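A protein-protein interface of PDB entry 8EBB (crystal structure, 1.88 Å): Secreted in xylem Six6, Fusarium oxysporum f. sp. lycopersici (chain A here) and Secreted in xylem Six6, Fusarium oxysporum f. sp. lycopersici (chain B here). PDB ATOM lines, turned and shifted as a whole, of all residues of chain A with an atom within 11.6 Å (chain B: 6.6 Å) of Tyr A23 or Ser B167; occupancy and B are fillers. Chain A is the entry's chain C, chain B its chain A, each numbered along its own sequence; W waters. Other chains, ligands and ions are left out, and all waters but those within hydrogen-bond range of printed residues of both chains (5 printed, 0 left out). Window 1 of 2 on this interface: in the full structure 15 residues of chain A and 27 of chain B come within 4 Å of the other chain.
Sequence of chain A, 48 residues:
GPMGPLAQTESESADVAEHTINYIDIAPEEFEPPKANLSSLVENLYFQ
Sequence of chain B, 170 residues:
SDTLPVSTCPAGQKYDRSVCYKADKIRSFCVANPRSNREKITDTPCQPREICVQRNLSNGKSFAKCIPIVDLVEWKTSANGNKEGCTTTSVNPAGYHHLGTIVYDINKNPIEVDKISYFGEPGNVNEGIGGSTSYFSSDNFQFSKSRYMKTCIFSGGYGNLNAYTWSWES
The guanidinium group (NH2) of Arg B55 lies within salt-bridge range of the side-chain carboxylate (OD2) of Asp A25, at 3.3 Å.
NZ of Lys B65 is in salt-bridge range of OD1 of Asp A25.
The backbone carbonyl oxygen of Ile A21 sits at hydrogen-bond distance from the backbone NH of Asn B92.
The side-chain amide oxygen of Asn A22 sits at hydrogen-bond distance from the side-chain amide nitrogen of Asn B92, at 2.9 Å.
The backbone carbonyl oxygen (O) of Ser B167 sits at hydrogen-bond distance from the backbone NH (N) of Asp A25 (2.8 Å).
The backbone NH (N) of Glu B169 sits at hydrogen-bond distance from the backbone carbonyl oxygen (O) of Asp A25 (3.0 Å).
The backbone NH (N) of Ala A27 lies close to the guanidinium group (NH2) of Arg B55.
The side-chain carboxylate of Glu B169 sits at hydrogen-bond distance from a ring nitrogen (ND1) of His B97, 2.4 Å away.
The backbone carbonyl oxygen of His B98 lies within hydrogen-bond range of the side-chain hydroxyl of Ser B167 (2.9 Å).
N of His B98 lies within hydrogen-bond range of O of Trp B168 (2.9 Å).
O of Trp B166 is in hydrogen-bond range of N of Gly B100, 2.8 Å away.
OH of Tyr A23 sits at hydrogen-bond distance from OD1 of Asp A25 (2.7 Å).
Val B91 touches Ile A21 (CA to O, 3.5 Å).
CD1 of Ile A21 touches O of Thr B165 (3.6 Å).
Trp B166 touches Ile A21 (CA to CD1, 3.96 Å).
Ser B167 touches Ile A21.
O of Tyr A23 touches CB of Ser B167 (3.9 Å).
CD1 of Ile A24 touches O of Asn B92 (3.6 Å).
His B97 touches Ile A24.
Ile A24 touches Ser B167 (CA to O, 3.6 Å).
OD1 of Asp A25 touches CD1 of Ile B67 (3.9 Å).
Asp A25 touches Trp B168.
Tyr A23 touches just these residues of chain B: Lys B65, Asp B71 and Ser B167.
Printed residues of chain B within 4 Å of Ile A24: Asn B92, His B97, Ser B167 and Glu B169.
Printed residues of chain B within 4 Å of Ile A26: Glu B169.
Printed residues of chain A within 4 Å of Ile B67: Asp A25.
No residue of chain A comes within 4 Å of Pro B68.
Of chain A, only Tyr A23 comes within 4 Å of Asp B71.
Printed residues of chain A within 4 Å of Asn B92: Thr A20, Ile A21, Asn A22 and Ile A24.
His B97 touches just one residue of chain A: Ile A24 (3.3 Å).
No residue of chain A comes within 4 Å of Leu B99.
Printed residues of chain A within 4 Å of Thr B165: Ile A21.
Trp B166 touches one residue of chain A.
Ser B167 touches just these residues of chain A: Ile A21, Tyr A23, Ile A24 and Asp A25.
The nearest residue of chain A that does not touch Ser B167 is Ile A26 (5.7 Å).
The nearest printed residue of chain B that does not touch Ile A24 is Trp B168 (4.01 Å).
Hydrophobic or aromatic side chains of chain A that line the printed part of chain B: Ile A21, Tyr A23, Ile A24 and Ile A26.
Of the 19 printed residues of chain B, 12 touch a printed residue of chain A.
Printed residues of chain B that touch a printed residue of chain A: Arg B55, Lys B65, Ile B67, Asp B71, Val B91, Asn B92, His B97, Thr B165, Trp B166, Ser B167, Trp B168 and Glu B169.
Among the printed residues, Asp or Glu carboxylates within 4 Å of a Lys or Arg side-chain nitrogen of the other chain: Asp A25 with Arg B55 (3.3 Å) and Asp A25 with Lys B65 (2.7 Å).
Water W1 lies within hydrogen-bond range of OE1 of Glu A32, O of Glu B169, N of Ala A27 and NH1 of Arg B55.
Water W5 lies within hydrogen-bond range of NE of Arg B55 (2.6 Å), OD2 of Asp A25 (3.0 Å) and NE1 of Trp B166 (3.1 Å).
Water W3 lies within hydrogen-bond range of the backbone carbonyl oxygen of Asn B92 (2.7 Å) and the backbone carbonyl oxygen of Asn A22 (2.9 Å).
Water W4 lies within hydrogen-bond range of the backbone carbonyl oxygen (O) of Tyr A23, the backbone carbonyl oxygen (O) of Asp B71 and the backbone NH (N) of Ser B167.
Water W2 lies within hydrogen-bond range of N of Asn A22 (2.8 Å) and O of Asp B71 (3.1 Å).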
ATOM      1  N   HIS A  19       4.307  21.579   7.872  1.00  0.00           N
ATOM      2  CA  HIS A  19       4.357  23.008   8.152  1.00  0.00           C
ATOM      3  C   HIS A  19       5.416  23.291   9.201  1.00  0.00           C
ATOM      4  O   HIS A  19       5.728  22.439  10.035  1.00  0.00           O
ATOM      5  CB  HIS A  19       3.016  23.559   8.672  1.00  0.00           C
ATOM      6  CG  HIS A  19       1.836  23.147   7.851  1.00  0.00           C
ATOM      7  ND1 HIS A  19       1.528  23.733   6.641  1.00  0.00           N
ATOM      8  CD2 HIS A  19       0.884  22.210   8.070  1.00  0.00           C
ATOM      9  CE1 HIS A  19       0.438  23.174   6.148  1.00  0.00           C
ATOM     10  NE2 HIS A  19       0.023  22.252   7.001  1.00  0.00           N
ATOM     11  N   THR A  20       5.943  24.510   9.178  1.00  0.00           N
ATOM     12  CA  THR A  20       6.857  24.980  10.208  1.00  0.00           C
ATOM     13  C   THR A  20       6.315  26.269  10.792  1.00  0.00           C
ATOM     14  O   THR A  20       5.973  27.191  10.046  1.00  0.00           O
ATOM     15  CB  THR A  20       8.252  25.199   9.640  1.00  0.00           C
ATOM     16  OG1 THR A  20       8.756  23.939   9.198  1.00  0.00           O
ATOM     17  CG2 THR A  20       9.182  25.776  10.699  1.00  0.00           C
ATOM     18  N   ILE A  21       6.211  26.322  12.116  1.00  0.00           N
ATOM     19  CA  ILE A  21       5.749  27.514  12.825  1.00  0.00           C
ATOM     20  C   ILE A  21       6.964  28.308  13.288  1.00  0.00           C
ATOM     21  O   ILE A  21       7.912  27.738  13.840  1.00  0.00           O
ATOM     22  CB  ILE A  21       4.835  27.140  14.004  1.00  0.00           C
ATOM     23  CG1 ILE A  21       3.436  26.805  13.472  1.00  0.00           C
ATOM     24  CG2 ILE A  21       4.731  28.306  14.990  1.00  0.00           C
ATOM     25  CD1 ILE A  21       2.454  26.337  14.545  1.00  0.00           C
ATOM     26  N   ASN A  22       6.946  29.626  13.054  1.00  0.00           N
ATOM     27  CA  ASN A  22       8.042  30.497  13.463  1.00  0.00           C
ATOM     28  C   ASN A  22       7.588  31.572  14.446  1.00  0.00           C
ATOM     29  O   ASN A  22       8.287  32.580  14.622  1.00  0.00           O
ATOM     30  CB  ASN A  22       8.699  31.148  12.241  1.00  0.00           C
ATOM     31  CG  ASN A  22       9.498  30.170  11.442  1.00  0.00           C
ATOM     32  OD1 ASN A  22      10.505  29.636  11.924  1.00  0.00           O
ATOM     33  ND2 ASN A  22       9.062  29.913  10.206  1.00  0.00           N
ATOM     34  N   TYR A  23       6.427  31.399  15.071  1.00  0.00           N
ATOM     35  CA  TYR A  23       5.923  32.362  16.044  1.00  0.00           C
ATOM     36  C   TYR A  23       5.419  31.583  17.249  1.00  0.00           C
ATOM     37  O   TYR A  23       4.621  30.648  17.090  1.00  0.00           O
ATOM     38  CB  TYR A  23       4.795  33.229  15.472  1.00  0.00           C
ATOM     39  CG  TYR A  23       4.117  33.994  16.582  1.00  0.00           C
ATOM     40  CD1 TYR A  23       4.751  35.080  17.182  1.00  0.00           C
ATOM     41  CD2 TYR A  23       2.890  33.582  17.093  1.00  0.00           C
ATOM     42  CE1 TYR A  23       4.159  35.775  18.221  1.00  0.00           C
ATOM     43  CE2 TYR A  23       2.295  34.266  18.147  1.00  0.00           C
ATOM     44  CZ  TYR A  23       2.941  35.359  18.701  1.00  0.00           C
ATOM     45  OH  TYR A  23       2.373  36.038  19.744  1.00  0.00           O
ATOM     46  N   ILE A  24       5.865  31.967  18.446  1.00  0.00           N
ATOM     47  CA  ILE A  24       5.498  31.276  19.679  1.00  0.00           C
ATOM     48  C   ILE A  24       4.776  32.261  20.595  1.00  0.00           C
ATOM     49  O   ILE A  24       5.377  33.240  21.058  1.00  0.00           O
ATOM     50  CB  ILE A  24       6.730  30.662  20.361  1.00  0.00           C
ATOM     51  CG1 ILE A  24       7.334  29.591  19.445  1.00  0.00           C
ATOM     52  CG2 ILE A  24       6.370  30.019  21.702  1.00  0.00           C
ATOM     53  CD1 ILE A  24       8.630  29.067  19.931  1.00  0.00           C
ATOM     54  N   ASP A  25       3.493  31.996  20.861  1.00  0.00           N
ATOM     55  CA  ASP A  25       2.669  32.903  21.651  1.00  0.00           C
ATOM     56  C   ASP A  25       2.948  32.753  23.135  1.00  0.00           C
ATOM     57  O   ASP A  25       3.070  31.639  23.648  1.00  0.00           O
ATOM     58  CB  ASP A  25       1.183  32.638  21.410  1.00  0.00           C
ATOM     59  CG  ASP A  25       0.321  33.804  21.839  1.00  0.00           C
ATOM     60  OD1 ASP A  25       0.474  34.875  21.217  1.00  0.00           O
ATOM     61  OD2 ASP A  25      -0.473  33.674  22.811  1.00  0.00           O
ATOM     62  N   ILE A  26       3.040  33.883  23.834  1.00  0.00           N
ATOM     63  CA  ILE A  26       3.148  33.892  25.289  1.00  0.00           C
ATOM     64  C   ILE A  26       2.156  34.921  25.818  1.00  0.00           C
ATOM     65  O   ILE A  26       2.137  36.063  25.341  1.00  0.00           O
ATOM     66  CB  ILE A  26       4.580  34.207  25.772  1.00  0.00           C
ATOM     67  CG1 ILE A  26       5.566  33.126  25.296  1.00  0.00           C
ATOM     68  CG2 ILE A  26       4.622  34.330  27.290  1.00  0.00           C
ATOM     69  CD1 ILE A  26       6.991  33.407  25.613  1.00  0.00           C
ATOM     70  N   ALA A  27       1.318  34.512  26.772  1.00  0.00           N
ATOM     71  CA  ALA A  27       0.315  35.425  27.327  1.00  0.00           C
ATOM     72  C   ALA A  27       0.994  36.500  28.168  1.00  0.00           C
ATOM     73  O   ALA A  27       1.948  36.207  28.896  1.00  0.00           O
ATOM     74  CB  ALA A  27      -0.701  34.668  28.184  1.00  0.00           C
ATOM     75  N   PRO A  28       0.540  37.755  28.087  1.00  0.00           N
ATOM     76  CA  PRO A  28       1.159  38.797  28.909  1.00  0.00           C
ATOM     77  C   PRO A  28       1.043  38.459  30.385  1.00  0.00           C
ATOM     78  O   PRO A  28       0.108  37.774  30.825  1.00  0.00           O
ATOM     79  CB  PRO A  28       0.369  40.067  28.553  1.00  0.00           C
ATOM     80  CG  PRO A  28      -0.225  39.791  27.211  1.00  0.00           C
ATOM     81  CD  PRO A  28      -0.458  38.292  27.146  1.00  0.00           C
ATOM     82  N   GLU A  32      -1.431  36.105  32.902  1.00  0.00           N
ATOM     83  CA  GLU A  32      -0.814  34.890  33.437  1.00  0.00           C
ATOM     84  C   GLU A  32       0.291  35.327  34.391  1.00  0.00           C
ATOM     85  O   GLU A  32       1.467  35.386  34.005  1.00  0.00           O
ATOM     86  CB  GLU A  32      -0.251  34.003  32.327  1.00  0.00           C
ATOM     87  CG  GLU A  32      -0.021  32.532  32.724  1.00  0.00           C
ATOM     88  CD  GLU A  32       0.404  31.649  31.555  1.00  0.00           C
ATOM     89  OE1 GLU A  32       1.159  32.131  30.673  1.00  0.00           O
ATOM     90  OE2 GLU A  32      -0.015  30.464  31.519  1.00  0.00           O
ATOM     91  N   ASP B   2      -1.649  39.356  18.290  1.00  0.00           N
ATOM     92  CA  ASP B   2      -1.416  40.787  18.364  1.00  0.00           C
ATOM     93  C   ASP B   2      -2.625  41.489  19.002  1.00  0.00           C
ATOM     94  O   ASP B   2      -2.440  42.372  19.829  1.00  0.00           O
ATOM     95  CB  ASP B   2      -1.124  41.363  16.974  1.00  0.00           C
ATOM     96  CG  ASP B   2      -1.087  42.884  16.967  1.00  0.00           C
ATOM     97  OD1 ASP B   2      -0.210  43.475  17.637  1.00  0.00           O
ATOM     98  OD2 ASP B   2      -1.970  43.493  16.325  1.00  0.00           O
ATOM     99  N   ARG B  55      -6.922  29.067  24.916  1.00  0.00           N
ATOM    100  CA  ARG B  55      -6.315  27.994  25.692  1.00  0.00           C
ATOM    101  C   ARG B  55      -6.535  28.322  27.154  1.00  0.00           C
ATOM    102  O   ARG B  55      -6.964  29.424  27.501  1.00  0.00           O
ATOM    103  CB  ARG B  55      -4.816  27.863  25.410  1.00  0.00           C
ATOM    104  CG  ARG B  55      -4.055  29.139  25.682  1.00  0.00           C
ATOM    105  CD  ARG B  55      -2.566  28.855  25.426  1.00  0.00           C
ATOM    106  NE  ARG B  55      -1.786  30.036  25.079  1.00  0.00           N
ATOM    107  CZ  ARG B  55      -1.006  30.678  25.944  1.00  0.00           C
ATOM    108  NH1 ARG B  55      -0.927  30.299  27.221  1.00  0.00           N
ATOM    109  NH2 ARG B  55      -0.256  31.703  25.510  1.00  0.00           N
ATOM    110  N   LYS B  65      -7.082  35.325  22.372  1.00  0.00           N
ATOM    111  CA  LYS B  65      -6.455  36.450  21.689  1.00  0.00           C
ATOM    112  C   LYS B  65      -6.380  36.124  20.202  1.00  0.00           C
ATOM    113  O   LYS B  65      -6.545  34.969  19.790  1.00  0.00           O
ATOM    114  CB  LYS B  65      -5.068  36.737  22.259  1.00  0.00           C
ATOM    115  CG  LYS B  65      -4.033  35.642  21.943  1.00  0.00           C
ATOM    116  CD  LYS B  65      -2.624  36.105  22.277  1.00  0.00           C
ATOM    117  CE  LYS B  65      -2.018  36.924  21.153  1.00  0.00           C
ATOM    118  NZ  LYS B  65      -0.647  37.341  21.502  1.00  0.00           N
ATOM    119  N   ILE B  67      -4.259  35.979  16.675  1.00  0.00           N
ATOM    120  CA  ILE B  67      -2.914  35.821  16.120  1.00  0.00           C
ATOM    121  C   ILE B  67      -3.051  35.936  14.605  1.00  0.00           C
ATOM    122  O   ILE B  67      -4.042  35.427  14.054  1.00  0.00           O
ATOM    123  CB  ILE B  67      -2.307  34.466  16.530  1.00  0.00           C
ATOM    124  CG1 ILE B  67      -2.002  34.429  18.027  1.00  0.00           C
ATOM    125  CG2 ILE B  67      -1.022  34.155  15.731  1.00  0.00           C
ATOM    126  CD1 ILE B  67      -1.537  33.020  18.483  1.00  0.00           C
ATOM    127  N   PRO B  68      -2.112  36.577  13.893  1.00  0.00           N
ATOM    128  CA  PRO B  68      -2.162  36.551  12.423  1.00  0.00           C
ATOM    129  C   PRO B  68      -2.162  35.120  11.896  1.00  0.00           C
ATOM    130  O   PRO B  68      -1.381  34.271  12.341  1.00  0.00           O
ATOM    131  CB  PRO B  68      -0.891  37.307  12.009  1.00  0.00           C
ATOM    132  CG  PRO B  68      -0.556  38.178  13.195  1.00  0.00           C
ATOM    133  CD  PRO B  68      -0.956  37.350  14.387  1.00  0.00           C
ATOM    134  N   ASP B  71       0.955  33.394  10.975  1.00  0.00           N
ATOM    135  CA  ASP B  71       1.832  32.950  12.052  1.00  0.00           C
ATOM    136  C   ASP B  71       1.426  31.610  12.663  1.00  0.00           C
ATOM    137  O   ASP B  71       2.055  31.179  13.631  1.00  0.00           O
ATOM    138  CB  ASP B  71       1.894  34.022  13.150  1.00  0.00           C
ATOM    139  CG  ASP B  71       2.530  35.331  12.657  1.00  0.00           C
ATOM    140  OD1 ASP B  71       3.367  35.275  11.734  1.00  0.00           O
ATOM    141  OD2 ASP B  71       2.203  36.407  13.201  1.00  0.00           O
ATOM    142  N   LEU B  72       0.398  30.946  12.138  1.00  0.00           N
ATOM    143  CA  LEU B  72       0.003  29.638  12.640  1.00  0.00           C
ATOM    144  C   LEU B  72      -0.384  28.775  11.446  1.00  0.00           C
ATOM    145  O   LEU B  72      -0.180  29.153  10.284  1.00  0.00           O
ATOM    146  CB  LEU B  72      -1.128  29.758  13.676  1.00  0.00           C
ATOM    147  CG  LEU B  72      -2.310  30.671  13.310  1.00  0.00           C
ATOM    148  CD1 LEU B  72      -3.214  30.068  12.248  1.00  0.00           C
ATOM    149  CD2 LEU B  72      -3.121  30.991  14.572  1.00  0.00           C
ATOM    150  N   VAL B  91       8.236  23.391  14.952  1.00  0.00           N
ATOM    151  CA  VAL B  91       8.249  24.712  15.579  1.00  0.00           C
ATOM    152  C   VAL B  91       9.689  25.159  15.781  1.00  0.00           C
ATOM    153  O   VAL B  91      10.492  24.431  16.380  1.00  0.00           O
ATOM    154  CB  VAL B  91       7.500  24.712  16.923  1.00  0.00           C
ATOM    155  CG1 VAL B  91       7.483  26.091  17.500  1.00  0.00           C
ATOM    156  CG2 VAL B  91       6.061  24.220  16.711  1.00  0.00           C
ATOM    157  N   ASN B  92      10.015  26.351  15.283  1.00  0.00           N
ATOM    158  CA  ASN B  92      11.311  27.014  15.450  1.00  0.00           C
ATOM    159  C   ASN B  92      11.234  28.047  16.565  1.00  0.00           C
ATOM    160  O   ASN B  92      10.214  28.729  16.698  1.00  0.00           O
ATOM    161  CB  ASN B  92      11.736  27.725  14.168  1.00  0.00           C
ATOM    162  CG  ASN B  92      12.204  26.774  13.106  1.00  0.00           C
ATOM    163  OD1 ASN B  92      12.790  25.724  13.397  1.00  0.00           O
ATOM    164  ND2 ASN B  92      11.942  27.126  11.856  1.00  0.00           N
ATOM    165  N   HIS B  97       7.967  23.530  23.615  1.00  0.00           N
ATOM    166  CA  HIS B  97       6.799  24.352  23.289  1.00  0.00           C
ATOM    167  C   HIS B  97       5.542  23.492  23.328  1.00  0.00           C
ATOM    168  O   HIS B  97       5.610  22.270  23.218  1.00  0.00           O
ATOM    169  CB  HIS B  97       6.858  24.994  21.883  1.00  0.00           C
ATOM    170  CG  HIS B  97       8.224  25.424  21.438  1.00  0.00           C
ATOM    171  ND1 HIS B  97       8.983  26.342  22.129  1.00  0.00           N
ATOM    172  CD2 HIS B  97       8.952  25.073  20.348  1.00  0.00           C
ATOM    173  CE1 HIS B  97      10.127  26.529  21.489  1.00  0.00           C
ATOM    174  NE2 HIS B  97      10.128  25.777  20.402  1.00  0.00           N
ATOM    175  N   HIS B  98       4.390  24.156  23.426  1.00  0.00           N
ATOM    176  CA  HIS B  98       3.083  23.536  23.236  1.00  0.00           C
ATOM    177  C   HIS B  98       2.546  23.865  21.841  1.00  0.00           C
ATOM    178  O   HIS B  98       2.916  24.868  21.232  1.00  0.00           O
ATOM    179  CB  HIS B  98       2.059  24.059  24.259  1.00  0.00           C
ATOM    180  CG  HIS B  98       2.421  23.829  25.693  1.00  0.00           C
ATOM    181  ND1 HIS B  98       1.923  22.776  26.432  1.00  0.00           N
ATOM    182  CD2 HIS B  98       3.197  24.547  26.538  1.00  0.00           C
ATOM    183  CE1 HIS B  98       2.386  22.851  27.669  1.00  0.00           C
ATOM    184  NE2 HIS B  98       3.159  23.917  27.760  1.00  0.00           N
ATOM    185  N   LEU B  99       1.596  23.058  21.380  1.00  0.00           N
ATOM    186  CA  LEU B  99       0.673  23.492  20.343  1.00  0.00           C
ATOM    187  C   LEU B  99      -0.707  23.676  20.961  1.00  0.00           C
ATOM    188  O   LEU B  99      -1.074  22.965  21.888  1.00  0.00           O
ATOM    189  CB  LEU B  99       0.563  22.471  19.216  1.00  0.00           C
ATOM    190  CG  LEU B  99       1.805  22.255  18.359  1.00  0.00           C
ATOM    191  CD1 LEU B  99       1.434  21.260  17.244  1.00  0.00           C
ATOM    192  CD2 LEU B  99       2.375  23.569  17.827  1.00  0.00           C
ATOM    193  N   GLY B 100      -1.469  24.637  20.443  1.00  0.00           N
ATOM    194  CA  GLY B 100      -2.885  24.670  20.748  1.00  0.00           C
ATOM    195  C   GLY B 100      -3.634  24.488  19.447  1.00  0.00           C
ATOM    196  O   GLY B 100      -3.052  24.672  18.365  1.00  0.00           O
ATOM    197  N   PHE B 143      10.572  20.245  20.793  1.00  0.00           N
ATOM    198  CA  PHE B 143      10.770  20.366  19.351  1.00  0.00           C
ATOM    199  C   PHE B 143      12.253  20.534  19.013  1.00  0.00           C
ATOM    200  O   PHE B 143      13.025  21.120  19.780  1.00  0.00           O
ATOM    201  CB  PHE B 143       9.993  21.572  18.811  1.00  0.00           C
ATOM    202  CG  PHE B 143       8.483  21.404  18.862  1.00  0.00           C
ATOM    203  CD1 PHE B 143       7.773  21.680  20.029  1.00  0.00           C
ATOM    204  CD2 PHE B 143       7.779  20.974  17.740  1.00  0.00           C
ATOM    205  CE1 PHE B 143       6.363  21.538  20.076  1.00  0.00           C
ATOM    206  CE2 PHE B 143       6.389  20.813  17.780  1.00  0.00           C
ATOM    207  CZ  PHE B 143       5.686  21.085  18.951  1.00  0.00           C
ATOM    208  N   THR B 165      -3.944  25.779  14.306  1.00  0.00           N
ATOM    209  CA  THR B 165      -2.973  25.214  15.241  1.00  0.00           C
ATOM    210  C   THR B 165      -1.787  26.162  15.366  1.00  0.00           C
ATOM    211  O   THR B 165      -1.169  26.532  14.355  1.00  0.00           O
ATOM    212  CB  THR B 165      -2.524  23.828  14.773  1.00  0.00           C
ATOM    213  OG1 THR B 165      -3.639  22.917  14.851  1.00  0.00           O
ATOM    214  CG2 THR B 165      -1.393  23.314  15.662  1.00  0.00           C
ATOM    215  N   TRP B 166      -1.490  26.575  16.597  1.00  0.00           N
ATOM    216  CA  TRP B 166      -0.491  27.597  16.875  1.00  0.00           C
ATOM    217  C   TRP B 166       0.435  27.050  17.950  1.00  0.00           C
ATOM    218  O   TRP B 166       0.121  26.046  18.597  1.00  0.00           O
ATOM    219  CB  TRP B 166      -1.148  28.931  17.316  1.00  0.00           C
ATOM    220  CG  TRP B 166      -1.770  28.947  18.705  1.00  0.00           C
ATOM    221  CD1 TRP B 166      -1.242  29.501  19.844  1.00  0.00           C
ATOM    222  CD2 TRP B 166      -3.059  28.420  19.080  1.00  0.00           C
ATOM    223  NE1 TRP B 166      -2.114  29.335  20.902  1.00  0.00           N
ATOM    224  CE2 TRP B 166      -3.234  28.675  20.458  1.00  0.00           C
ATOM    225  CE3 TRP B 166      -4.075  27.753  18.381  1.00  0.00           C
ATOM    226  CZ2 TRP B 166      -4.385  28.269  21.163  1.00  0.00           C
ATOM    227  CZ3 TRP B 166      -5.219  27.354  19.078  1.00  0.00           C
ATOM    228  CH2 TRP B 166      -5.367  27.627  20.455  1.00  0.00           C
ATOM    229  N   SER B 167       1.568  27.716  18.165  1.00  0.00           N
ATOM    230  CA  SER B 167       2.486  27.312  19.231  1.00  0.00           C
ATOM    231  C   SER B 167       2.483  28.333  20.369  1.00  0.00           C
ATOM    232  O   SER B 167       2.326  29.538  20.138  1.00  0.00           O
ATOM    233  CB  SER B 167       3.919  27.128  18.703  1.00  0.00           C
ATOM    234  OG  SER B 167       4.741  26.585  19.727  1.00  0.00           O
ATOM    235  N   TRP B 168       2.666  27.845  21.604  1.00  0.00           N
ATOM    236  CA  TRP B 168       2.672  28.731  22.762  1.00  0.00           C
ATOM    237  C   TRP B 168       3.558  28.160  23.865  1.00  0.00           C
ATOM    238  O   TRP B 168       3.839  26.960  23.908  1.00  0.00           O
ATOM    239  CB  TRP B 168       1.237  28.995  23.290  1.00  0.00           C
ATOM    240  CG  TRP B 168       0.475  27.766  23.858  1.00  0.00           C
ATOM    241  CD1 TRP B 168      -0.406  26.945  23.183  1.00  0.00           C
ATOM    242  CD2 TRP B 168       0.516  27.277  25.210  1.00  0.00           C
ATOM    243  NE1 TRP B 168      -0.889  25.968  24.031  1.00  0.00           N
ATOM    244  CE2 TRP B 168      -0.334  26.144  25.275  1.00  0.00           C
ATOM    245  CE3 TRP B 168       1.212  27.669  26.365  1.00  0.00           C
ATOM    246  CZ2 TRP B 168      -0.516  25.411  26.452  1.00  0.00           C
ATOM    247  CZ3 TRP B 168       1.025  26.937  27.543  1.00  0.00           C
ATOM    248  CH2 TRP B 168       0.164  25.825  27.575  1.00  0.00           C
ATOM    249  N   GLU B 169       4.010  29.052  24.743  1.00  0.00           N
ATOM    250  CA  GLU B 169       4.763  28.717  25.944  1.00  0.00           C
ATOM    251  C   GLU B 169       4.164  29.458  27.130  1.00  0.00           C
ATOM    252  O   GLU B 169       3.494  30.479  26.972  1.00  0.00           O
ATOM    253  CB  GLU B 169       6.253  29.096  25.813  1.00  0.00           C
ATOM    254  CG  GLU B 169       7.024  28.245  24.815  1.00  0.00           C
ATOM    255  CD  GLU B 169       8.449  28.773  24.559  1.00  0.00           C
ATOM    256  OE1 GLU B 169       8.884  29.686  25.291  1.00  0.00           O
ATOM    257  OE2 GLU B 169       9.133  28.256  23.641  1.00  0.00           O
HETATM  258  O   HOH W   1       1.774  31.992  28.190  1.00  0.00           O
HETATM  259  O   HOH W   2       4.732  30.915  12.010  1.00  0.00           O
HETATM  260  O   HOH W   3       9.800  31.358  16.814  1.00  0.00           O
HETATM  261  O   HOH W   4       2.078  30.087  16.337  1.00  0.00           O
HETATM  262  O   HOH W   5      -2.488  31.500  23.069  1.00  0.00           O
